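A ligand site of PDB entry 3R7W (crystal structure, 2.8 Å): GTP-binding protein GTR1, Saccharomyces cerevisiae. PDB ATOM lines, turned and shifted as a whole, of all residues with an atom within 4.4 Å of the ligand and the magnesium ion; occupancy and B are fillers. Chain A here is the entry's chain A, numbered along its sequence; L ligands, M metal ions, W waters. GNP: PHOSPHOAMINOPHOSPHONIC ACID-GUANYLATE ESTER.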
ATOM      1  N   GLY A  10      -0.159  -9.053  -1.602  1.00  0.00           N
ATOM      2  CA  GLY A  10       0.242  -9.567  -0.314  1.00  0.00           C
ATOM      3  C   GLY A  10       1.257  -8.663   0.338  1.00  0.00           C
ATOM      4  O   GLY A  10       1.976  -7.937  -0.328  1.00  0.00           O
ATOM      5  N   ARG A  11       1.327  -8.729   1.653  1.00  0.00           N
ATOM      6  CA  ARG A  11       2.142  -7.761   2.359  1.00  0.00           C
ATOM      7  C   ARG A  11       3.642  -7.842   1.991  1.00  0.00           C
ATOM      8  O   ARG A  11       4.098  -8.855   1.441  1.00  0.00           O
ATOM      9  CB  ARG A  11       1.867  -7.848   3.874  1.00  0.00           C
ATOM     10  CG  ARG A  11       0.370  -7.573   4.245  1.00  0.00           C
ATOM     11  CD  ARG A  11       0.269  -6.384   5.180  1.00  0.00           C
ATOM     12  NE  ARG A  11       1.216  -6.587   6.287  1.00  0.00           N
ATOM     13  CZ  ARG A  11       1.351  -5.779   7.324  1.00  0.00           C
ATOM     14  NH1 ARG A  11       0.605  -4.678   7.439  1.00  0.00           N
ATOM     15  NH2 ARG A  11       2.258  -6.064   8.267  1.00  0.00           N
ATOM     16  N   SER A  12       4.378  -6.752   2.232  1.00  0.00           N
ATOM     17  CA  SER A  12       5.766  -6.673   1.792  1.00  0.00           C
ATOM     18  C   SER A  12       6.587  -7.765   2.443  1.00  0.00           C
ATOM     19  O   SER A  12       6.259  -8.209   3.538  1.00  0.00           O
ATOM     20  CB  SER A  12       6.377  -5.308   2.089  1.00  0.00           C
ATOM     21  OG  SER A  12       7.800  -5.392   1.997  1.00  0.00           O
ATOM     22  N   GLY A  13       7.668  -8.175   1.766  1.00  0.00           N
ATOM     23  CA  GLY A  13       8.528  -9.238   2.245  1.00  0.00           C
ATOM     24  C   GLY A  13       7.945 -10.648   2.227  1.00  0.00           C
ATOM     25  O   GLY A  13       8.682 -11.623   2.435  1.00  0.00           O
ATOM     26  N   SER A  14       6.641 -10.781   1.981  1.00  0.00           N
ATOM     27  CA  SER A  14       6.030 -12.127   1.940  1.00  0.00           C
ATOM     28  C   SER A  14       6.577 -13.053   0.864  1.00  0.00           C
ATOM     29  O   SER A  14       6.389 -14.263   0.931  1.00  0.00           O
ATOM     30  CB  SER A  14       4.524 -12.037   1.773  1.00  0.00           C
ATOM     31  OG  SER A  14       4.218 -11.436   0.547  1.00  0.00           O
ATOM     32  N   GLY A  15       7.231 -12.496  -0.151  1.00  0.00           N
ATOM     33  CA  GLY A  15       7.901 -13.292  -1.159  1.00  0.00           C
ATOM     34  C   GLY A  15       7.220 -13.393  -2.516  1.00  0.00           C
ATOM     35  O   GLY A  15       7.480 -14.333  -3.252  1.00  0.00           O
ATOM     36  N   LYS A  16       6.357 -12.435  -2.841  1.00  0.00           N
ATOM     37  CA  LYS A  16       5.603 -12.444  -4.078  1.00  0.00           C
ATOM     38  C   LYS A  16       6.461 -12.367  -5.357  1.00  0.00           C
ATOM     39  O   LYS A  16       6.220 -13.110  -6.309  1.00  0.00           O
ATOM     40  CB  LYS A  16       4.557 -11.333  -4.084  1.00  0.00           C
ATOM     41  CG  LYS A  16       3.564 -11.429  -2.967  1.00  0.00           C
ATOM     42  CD  LYS A  16       2.534 -10.323  -3.085  1.00  0.00           C
ATOM     43  CE  LYS A  16       3.207  -8.985  -3.221  1.00  0.00           C
ATOM     44  NZ  LYS A  16       4.094  -8.775  -2.054  1.00  0.00           N
ATOM     45  N   SER A  17       7.432 -11.457  -5.386  1.00  0.00           N
ATOM     46  CA  SER A  17       8.295 -11.318  -6.565  1.00  0.00           C
ATOM     47  C   SER A  17       9.128 -12.568  -6.767  1.00  0.00           C
ATOM     48  O   SER A  17       9.243 -13.087  -7.860  1.00  0.00           O
ATOM     49  CB  SER A  17       9.189 -10.097  -6.446  1.00  0.00           C
ATOM     50  OG  SER A  17       8.406  -8.936  -6.485  1.00  0.00           O
ATOM     51  N   SER A  18       9.710 -13.044  -5.681  1.00  0.00           N
ATOM     52  CA  SER A  18      10.393 -14.318  -5.681  1.00  0.00           C
ATOM     53  C   SER A  18       9.676 -15.381  -6.480  1.00  0.00           C
ATOM     54  O   SER A  18      10.270 -15.972  -7.374  1.00  0.00           O
ATOM     55  CB  SER A  18      10.540 -14.784  -4.240  1.00  0.00           C
ATOM     56  OG  SER A  18      11.817 -14.401  -3.785  1.00  0.00           O
ATOM     57  N   THR A  32      16.936 -15.247  -5.801  1.00  0.00           N
ATOM     58  CA  THR A  32      15.802 -14.373  -5.449  1.00  0.00           C
ATOM     59  C   THR A  32      16.110 -13.316  -4.399  1.00  0.00           C
ATOM     60  O   THR A  32      15.336 -12.384  -4.225  1.00  0.00           O
ATOM     61  CB  THR A  32      14.537 -15.154  -4.985  1.00  0.00           C
ATOM     62  OG1 THR A  32      14.842 -15.981  -3.854  1.00  0.00           O
ATOM     63  CG2 THR A  32      13.992 -16.020  -6.109  1.00  0.00           C
ATOM     64  N   ARG A  33      17.233 -13.461  -3.690  1.00  0.00           N
ATOM     65  CA  ARG A  33      17.537 -12.525  -2.605  1.00  0.00           C
ATOM     66  C   ARG A  33      17.757 -11.090  -3.097  1.00  0.00           C
ATOM     67  O   ARG A  33      17.429 -10.140  -2.385  1.00  0.00           O
ATOM     68  CB  ARG A  33      18.703 -13.020  -1.726  1.00  0.00           C
ATOM     69  CG  ARG A  33      20.038 -13.327  -2.447  1.00  0.00           C
ATOM     70  CD  ARG A  33      20.681 -14.633  -1.927  1.00  0.00           C
ATOM     71  NE  ARG A  33      20.507 -14.799  -0.480  1.00  0.00           N
ATOM     72  CZ  ARG A  33      20.228 -15.958   0.135  1.00  0.00           C
ATOM     73  NH1 ARG A  33      20.071 -17.078  -0.549  1.00  0.00           N
ATOM     74  NH2 ARG A  33      20.089 -15.981   1.454  1.00  0.00           N
ATOM     75  N   LEU A  35      16.281  -9.475  -5.524  1.00  0.00           N
ATOM     76  CA  LEU A  35      15.065  -8.800  -5.964  1.00  0.00           C
ATOM     77  C   LEU A  35      14.845  -7.637  -4.999  1.00  0.00           C
ATOM     78  O   LEU A  35      14.872  -7.829  -3.786  1.00  0.00           O
ATOM     79  CB  LEU A  35      13.885  -9.772  -5.870  1.00  0.00           C
ATOM     80  CG  LEU A  35      13.327 -10.601  -7.031  1.00  0.00           C
ATOM     81  CD1 LEU A  35      14.187 -10.573  -8.226  1.00  0.00           C
ATOM     82  CD2 LEU A  35      13.067 -12.019  -6.545  1.00  0.00           C
ATOM     83  N   GLY A  36      14.635  -6.441  -5.508  1.00  0.00           N
ATOM     84  CA  GLY A  36      14.405  -5.303  -4.625  1.00  0.00           C
ATOM     85  C   GLY A  36      12.957  -5.226  -4.173  1.00  0.00           C
ATOM     86  O   GLY A  36      12.205  -6.161  -4.372  1.00  0.00           O
ATOM     87  N   ALA A  37      12.554  -4.140  -3.552  1.00  0.00           N
ATOM     88  CA  ALA A  37      11.148  -3.998  -3.243  1.00  0.00           C
ATOM     89  C   ALA A  37      10.503  -3.643  -4.561  1.00  0.00           C
ATOM     90  O   ALA A  37      11.138  -3.114  -5.450  1.00  0.00           O
ATOM     91  CB  ALA A  37      10.900  -2.929  -2.191  1.00  0.00           C
ATOM     92  N   THR A  38       9.224  -3.945  -4.672  1.00  0.00           N
ATOM     93  CA  THR A  38       8.495  -3.659  -5.889  1.00  0.00           C
ATOM     94  C   THR A  38       7.798  -2.331  -5.711  1.00  0.00           C
ATOM     95  O   THR A  38       7.057  -2.147  -4.745  1.00  0.00           O
ATOM     96  CB  THR A  38       7.459  -4.778  -6.164  1.00  0.00           C
ATOM     97  OG1 THR A  38       8.143  -6.015  -6.387  1.00  0.00           O
ATOM     98  CG2 THR A  38       6.581  -4.425  -7.368  1.00  0.00           C
ATOM     99  N   ASP A  58       2.135  -7.811 -10.254  1.00  0.00           N
ATOM    100  CA  ASP A  58       2.830  -8.102  -9.025  1.00  0.00           C
ATOM    101  C   ASP A  58       2.827  -6.847  -8.169  1.00  0.00           C
ATOM    102  O   ASP A  58       3.764  -6.041  -8.251  1.00  0.00           O
ATOM    103  CB  ASP A  58       4.256  -8.561  -9.329  1.00  0.00           C
ATOM    104  CG  ASP A  58       5.057  -8.754  -8.085  1.00  0.00           C
ATOM    105  OD1 ASP A  58       4.535  -8.343  -7.038  1.00  0.00           O
ATOM    106  OD2 ASP A  58       6.193  -9.309  -8.152  1.00  0.00           O
ATOM    107  N   GLY A  60       3.260  -4.252  -5.367  1.00  0.00           N
ATOM    108  CA  GLY A  60       4.134  -3.983  -4.242  1.00  0.00           C
ATOM    109  C   GLY A  60       3.301  -4.001  -2.986  1.00  0.00           C
ATOM    110  O   GLY A  60       2.191  -3.481  -2.942  1.00  0.00           O
ATOM    111  N   GLY A  61       3.815  -4.629  -1.940  1.00  0.00           N
ATOM    112  CA  GLY A  61       3.011  -4.818  -0.738  1.00  0.00           C
ATOM    113  C   GLY A  61       3.156  -3.815   0.399  1.00  0.00           C
ATOM    114  O   GLY A  61       2.324  -3.810   1.303  1.00  0.00           O
ATOM    115  N   GLN A  62       4.182  -2.992   0.373  1.00  0.00           N
ATOM    116  CA  GLN A  62       4.355  -1.982   1.392  1.00  0.00           C
ATOM    117  C   GLN A  62       3.086  -1.158   1.585  1.00  0.00           C
ATOM    118  O   GLN A  62       2.262  -1.014   0.661  1.00  0.00           O
ATOM    119  CB  GLN A  62       5.490  -1.058   1.025  1.00  0.00           C
ATOM    120  CG  GLN A  62       6.838  -1.669   1.068  1.00  0.00           C
ATOM    121  CD  GLN A  62       7.816  -0.749   0.411  1.00  0.00           C
ATOM    122  OE1 GLN A  62       8.293  -1.019  -0.688  1.00  0.00           O
ATOM    123  NE2 GLN A  62       8.076   0.381   1.047  1.00  0.00           N
ATOM    124  N   HIS A 123       2.990 -18.727   2.664  1.00  0.00           N
ATOM    125  CA  HIS A 123       4.330 -18.812   2.058  1.00  0.00           C
ATOM    126  C   HIS A 123       5.493 -18.818   3.050  1.00  0.00           C
ATOM    127  O   HIS A 123       5.328 -18.524   4.216  1.00  0.00           O
ATOM    128  CB  HIS A 123       4.482 -17.735   0.954  1.00  0.00           C
ATOM    129  CG  HIS A 123       5.715 -17.883   0.119  1.00  0.00           C
ATOM    130  ND1 HIS A 123       6.163 -19.105  -0.322  1.00  0.00           N
ATOM    131  CD2 HIS A 123       6.608 -16.966  -0.315  1.00  0.00           C
ATOM    132  CE1 HIS A 123       7.286 -18.937  -1.004  1.00  0.00           C
ATOM    133  NE2 HIS A 123       7.572 -17.647  -1.019  1.00  0.00           N
ATOM    134  N   LYS A 124       6.687 -19.170   2.581  1.00  0.00           N
ATOM    135  CA  LYS A 124       7.874 -19.184   3.429  1.00  0.00           C
ATOM    136  C   LYS A 124       7.820 -20.302   4.473  1.00  0.00           C
ATOM    137  O   LYS A 124       8.291 -20.156   5.582  1.00  0.00           O
ATOM    138  CB  LYS A 124       8.032 -17.830   4.072  1.00  0.00           C
ATOM    139  CG  LYS A 124       9.048 -16.962   3.391  1.00  0.00           C
ATOM    140  CD  LYS A 124       8.839 -15.526   3.790  1.00  0.00           C
ATOM    141  CE  LYS A 124       9.961 -14.663   3.269  1.00  0.00           C
ATOM    142  NZ  LYS A 124       9.742 -13.288   3.809  1.00  0.00           N
ATOM    143  N   ASP A 126       9.274 -23.081   4.923  1.00  0.00           N
ATOM    144  CA  ASP A 126      10.507 -23.770   5.290  1.00  0.00           C
ATOM    145  C   ASP A 126      11.160 -23.183   6.564  1.00  0.00           C
ATOM    146  O   ASP A 126      12.186 -23.665   7.036  1.00  0.00           O
ATOM    147  CB  ASP A 126      11.490 -23.645   4.125  1.00  0.00           C
ATOM    148  CG  ASP A 126      11.791 -22.209   3.810  1.00  0.00           C
ATOM    149  OD1 ASP A 126      10.881 -21.533   3.294  1.00  0.00           O
ATOM    150  OD2 ASP A 126      12.910 -21.741   4.091  1.00  0.00           O
ATOM    151  N   LEU A 127      10.569 -22.099   7.067  1.00  0.00           N
ATOM    152  CA  LEU A 127      10.971 -21.463   8.305  1.00  0.00           C
ATOM    153  C   LEU A 127      10.135 -22.009   9.481  1.00  0.00           C
ATOM    154  O   LEU A 127      10.272 -21.494  10.598  1.00  0.00           O
ATOM    155  CB  LEU A 127      10.767 -19.949   8.240  1.00  0.00           C
ATOM    156  CG  LEU A 127      11.397 -19.124   7.113  1.00  0.00           C
ATOM    157  CD1 LEU A 127      10.907 -17.694   7.183  1.00  0.00           C
ATOM    158  CD2 LEU A 127      12.905 -19.184   7.141  1.00  0.00           C
ATOM    159  N   SER A 162       6.660 -23.053  -0.561  1.00  0.00           N
ATOM    160  CA  SER A 162       7.996 -22.555  -0.286  1.00  0.00           C
ATOM    161  C   SER A 162       8.890 -22.446  -1.507  1.00  0.00           C
ATOM    162  O   SER A 162       8.738 -23.165  -2.486  1.00  0.00           O
ATOM    163  CB  SER A 162       8.696 -23.420   0.748  1.00  0.00           C
ATOM    164  OG  SER A 162      10.025 -22.955   0.887  1.00  0.00           O
ATOM    165  N   ILE A 163       9.833 -21.532  -1.416  1.00  0.00           N
ATOM    166  CA  ILE A 163      10.822 -21.301  -2.450  1.00  0.00           C
ATOM    167  C   ILE A 163      11.827 -22.470  -2.478  1.00  0.00           C
ATOM    168  O   ILE A 163      12.499 -22.701  -3.492  1.00  0.00           O
ATOM    169  CB  ILE A 163      11.516 -19.927  -2.163  1.00  0.00           C
ATOM    170  CG1 ILE A 163      11.397 -19.064  -3.390  1.00  0.00           C
ATOM    171  CG2 ILE A 163      12.973 -20.042  -1.655  1.00  0.00           C
ATOM    172  CD1 ILE A 163      10.115 -19.320  -4.059  1.00  0.00           C
ATOM    173  N   TRP A 164      11.908 -23.210  -1.368  1.00  0.00           N
ATOM    174  CA  TRP A 164      13.012 -24.155  -1.153  1.00  0.00           C
ATOM    175  C   TRP A 164      12.602 -25.599  -1.329  1.00  0.00           C
ATOM    176  O   TRP A 164      13.374 -26.498  -0.980  1.00  0.00           O
ATOM    177  CB  TRP A 164      13.650 -23.942   0.241  1.00  0.00           C
ATOM    178  CG  TRP A 164      14.353 -22.617   0.372  1.00  0.00           C
ATOM    179  CD1 TRP A 164      13.941 -21.539   1.073  1.00  0.00           C
ATOM    180  CD2 TRP A 164      15.596 -22.258  -0.238  1.00  0.00           C
ATOM    181  NE1 TRP A 164      14.841 -20.510   0.938  1.00  0.00           N
ATOM    182  CE2 TRP A 164      15.870 -20.918   0.134  1.00  0.00           C
ATOM    183  CE3 TRP A 164      16.508 -22.916  -1.074  1.00  0.00           C
ATOM    184  CZ2 TRP A 164      16.999 -20.237  -0.301  1.00  0.00           C
ATOM    185  CZ3 TRP A 164      17.636 -22.235  -1.509  1.00  0.00           C
ATOM    186  CH2 TRP A 164      17.874 -20.914  -1.108  1.00  0.00           C
HETATM  187  PG  GNP L   1       7.348  -6.602  -1.836  1.00  0.00           P
HETATM  188  O1G GNP L   1       7.847  -6.336  -3.237  1.00  0.00           O
HETATM  189  O2G GNP L   1       7.456  -5.362  -1.009  1.00  0.00           O
HETATM  190  O3G GNP L   1       5.924  -7.075  -1.830  1.00  0.00           O
HETATM  191  N3B GNP L   1       8.277  -7.832  -1.317  1.00  0.00           N
HETATM  192  PB  GNP L   1       8.092  -9.322  -1.913  1.00  0.00           P
HETATM  193  O1B GNP L   1       6.727  -9.782  -1.555  1.00  0.00           O
HETATM  194  O2B GNP L   1       8.383  -9.184  -3.371  1.00  0.00           O
HETATM  195  O3A GNP L   1       9.077 -10.413  -1.392  1.00  0.00           O
HETATM  196  PA  GNP L   1      10.395 -10.760  -2.126  1.00  0.00           P
HETATM  197  O1A GNP L   1      10.252 -12.108  -2.701  1.00  0.00           O
HETATM  198  O2A GNP L   1      10.765  -9.614  -2.986  1.00  0.00           O
HETATM  199  O5' GNP L   1      11.651 -10.908  -1.156  1.00  0.00           O
HETATM  200  C5' GNP L   1      11.378 -11.456   0.117  1.00  0.00           C
HETATM  201  C4' GNP L   1      12.558 -12.156   0.710  1.00  0.00           C
HETATM  202  O4' GNP L   1      12.172 -13.472   1.149  1.00  0.00           O
HETATM  203  C3' GNP L   1      13.722 -12.394  -0.213  1.00  0.00           C
HETATM  204  O3' GNP L   1      14.799 -12.320   0.651  1.00  0.00           O
HETATM  205  C2' GNP L   1      13.536 -13.831  -0.724  1.00  0.00           C
HETATM  206  O2' GNP L   1      14.740 -14.528  -0.965  1.00  0.00           O
HETATM  207  C1' GNP L   1      12.922 -14.498   0.485  1.00  0.00           C
HETATM  208  N9  GNP L   1      11.981 -15.584   0.239  1.00  0.00           N
HETATM  209  C8  GNP L   1      10.942 -15.649  -0.656  1.00  0.00           C
HETATM  210  N7  GNP L   1      10.258 -16.755  -0.553  1.00  0.00           N
HETATM  211  C5  GNP L   1      10.870 -17.453   0.478  1.00  0.00           C
HETATM  212  C6  GNP L   1      10.582 -18.708   1.059  1.00  0.00           C
HETATM  213  O6  GNP L   1       9.703 -19.533   0.771  1.00  0.00           O
HETATM  214  N1  GNP L   1      11.446 -19.027   2.099  1.00  0.00           N
HETATM  215  C2  GNP L   1      12.478 -18.239   2.528  1.00  0.00           C
HETATM  216  N2  GNP L   1      13.195 -18.767   3.528  1.00  0.00           N
HETATM  217  N3  GNP L   1      12.768 -17.055   1.995  1.00  0.00           N
HETATM  218  C4  GNP L   1      11.927 -16.730   0.983  1.00  0.00           C
HETATM  219 MG    MG M   1       8.180  -7.697  -4.863  1.00  0.00          MG
HETATM  220  O   HOH W   1      10.175  -7.597  -4.570  1.00  0.00           O
HETATM  221  O   HOH W   2       6.046  -7.903  -5.201  1.00  0.00           O
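An oxygen (O1A) of the ligand sits close to the backbone NH (N) of Ser 18.
An oxygen (O3A) of the ligand is in hydrogen-bond range of the backbone NH (N) of Gly 15, 3.0 Å away.
The backbone NH (N) of Thr 38 sits close to an oxygen (O1G) of the ligand (3.1 Å).
A ring nitrogen (NE2) of His 123 sits at hydrogen-bond distance from a nitrogen (N7) of the ligand, at 2.9 Å.
A nitrogen (N1) of the ligand sits at hydrogen-bond distance from the side-chain carboxylate (OD1) of Asp 126 (2.8 Å).
O6 of the ligand is in hydrogen-bond range of N of Ile 163 (3.0 Å).
NZ of Lys 16 lies within salt-bridge range of O3G of the ligand (2.5 Å).
An oxygen (O2G) of the ligand is in hydrogen-bond range of the side-chain hydroxyl (OG) of Ser 12.
An oxygen (O2') of the ligand is in hydrogen-bond range of the side-chain hydroxyl of Thr 32.
OG of Ser 162 lies within hydrogen-bond range of O6 of the ligand (3.4 Å).
N of Ser 17 lies close to O2B of the ligand (3.2 Å).
N of Lys 16 lies within hydrogen-bond range of O1B of the ligand (3.0 Å).
An oxygen (O1A) of the ligand is in hydrogen-bond range of the side-chain hydroxyl of Ser 18 (3.0 Å).
An oxygen (O3G) of the ligand is in hydrogen-bond range of the backbone NH (N) of Gly 61, 3.2 Å away.
O of Arg 11 is in hydrogen-bond range of NZ of Lys 16.
The backbone carbonyl oxygen (O) of Gly 13 sits at hydrogen-bond distance from the side-chain amino group (NZ) of Lys 124, 2.4 Å away.
OG of Ser 17 lies close to OD2 of Asp 58.
The backbone NH (N) of Trp 164 sits at hydrogen-bond distance from the side-chain hydroxyl (OG) of Ser 162, 2.9 Å away.
The side-chain carboxylate (OD1) of Asp 126 lies within hydrogen-bond range of the side-chain hydroxyl (OG) of Ser 162 (2.9 Å).
O of Arg 11 lies within hydrogen-bond range of OG of Ser 14 (2.7 Å).
The backbone carbonyl oxygen (O) of Gly 10 lies within hydrogen-bond range of the side-chain amino group (NZ) of Lys 16 (2.9 Å).
OG of Ser 18 sits close to OG1 of Thr 32 (3.4 Å).
The backbone NH (N) of Gly 13 lies close to a nitrogen (N3B) of the ligand (3.2 Å).
Ser 14 touches the ligand (OG to O1B, 3.7 Å).
Arg 33 touches the ligand.
Gly 36 touches the ligand (O to O2A, 3.99 Å).
CA of Lys 124 touches O6 of the ligand, at 3.2 Å.
Leu 127 touches the ligand (CD2 to N2, 3.6 Å).
Trp 164 touches the ligand (NE1 to N2, 3.5 Å).
Hydrophobic or aromatic side chains that line the ligand: His 123, Leu 127, Ile 163 and Trp 164.
Of the 26 residues printed, 19 come within 4 Å of the ligand.
Of the 26 residues printed, 2 come within 4 Å of the magnesium ion.
The magnesium ion is bound by water W1 (2.0 Å), OG of Ser 17 (2.1 Å), O2B of the ligand (2.1 Å), O1G of the ligand (2.1 Å), water W2 (2.2 Å) and OG1 of Thr 38 (2.3 Å).
Water W1 lies within hydrogen-bond range of the backbone carbonyl oxygen (O) of Gly 36 (2.5 Å) and an oxygen (O2A) of the ligand (2.6 Å).
Water W2 lies within hydrogen-bond range of the side-chain carboxylate of Asp 58 (2.4 Å) and an oxygen (O3G) of the ligand (3.5 Å).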
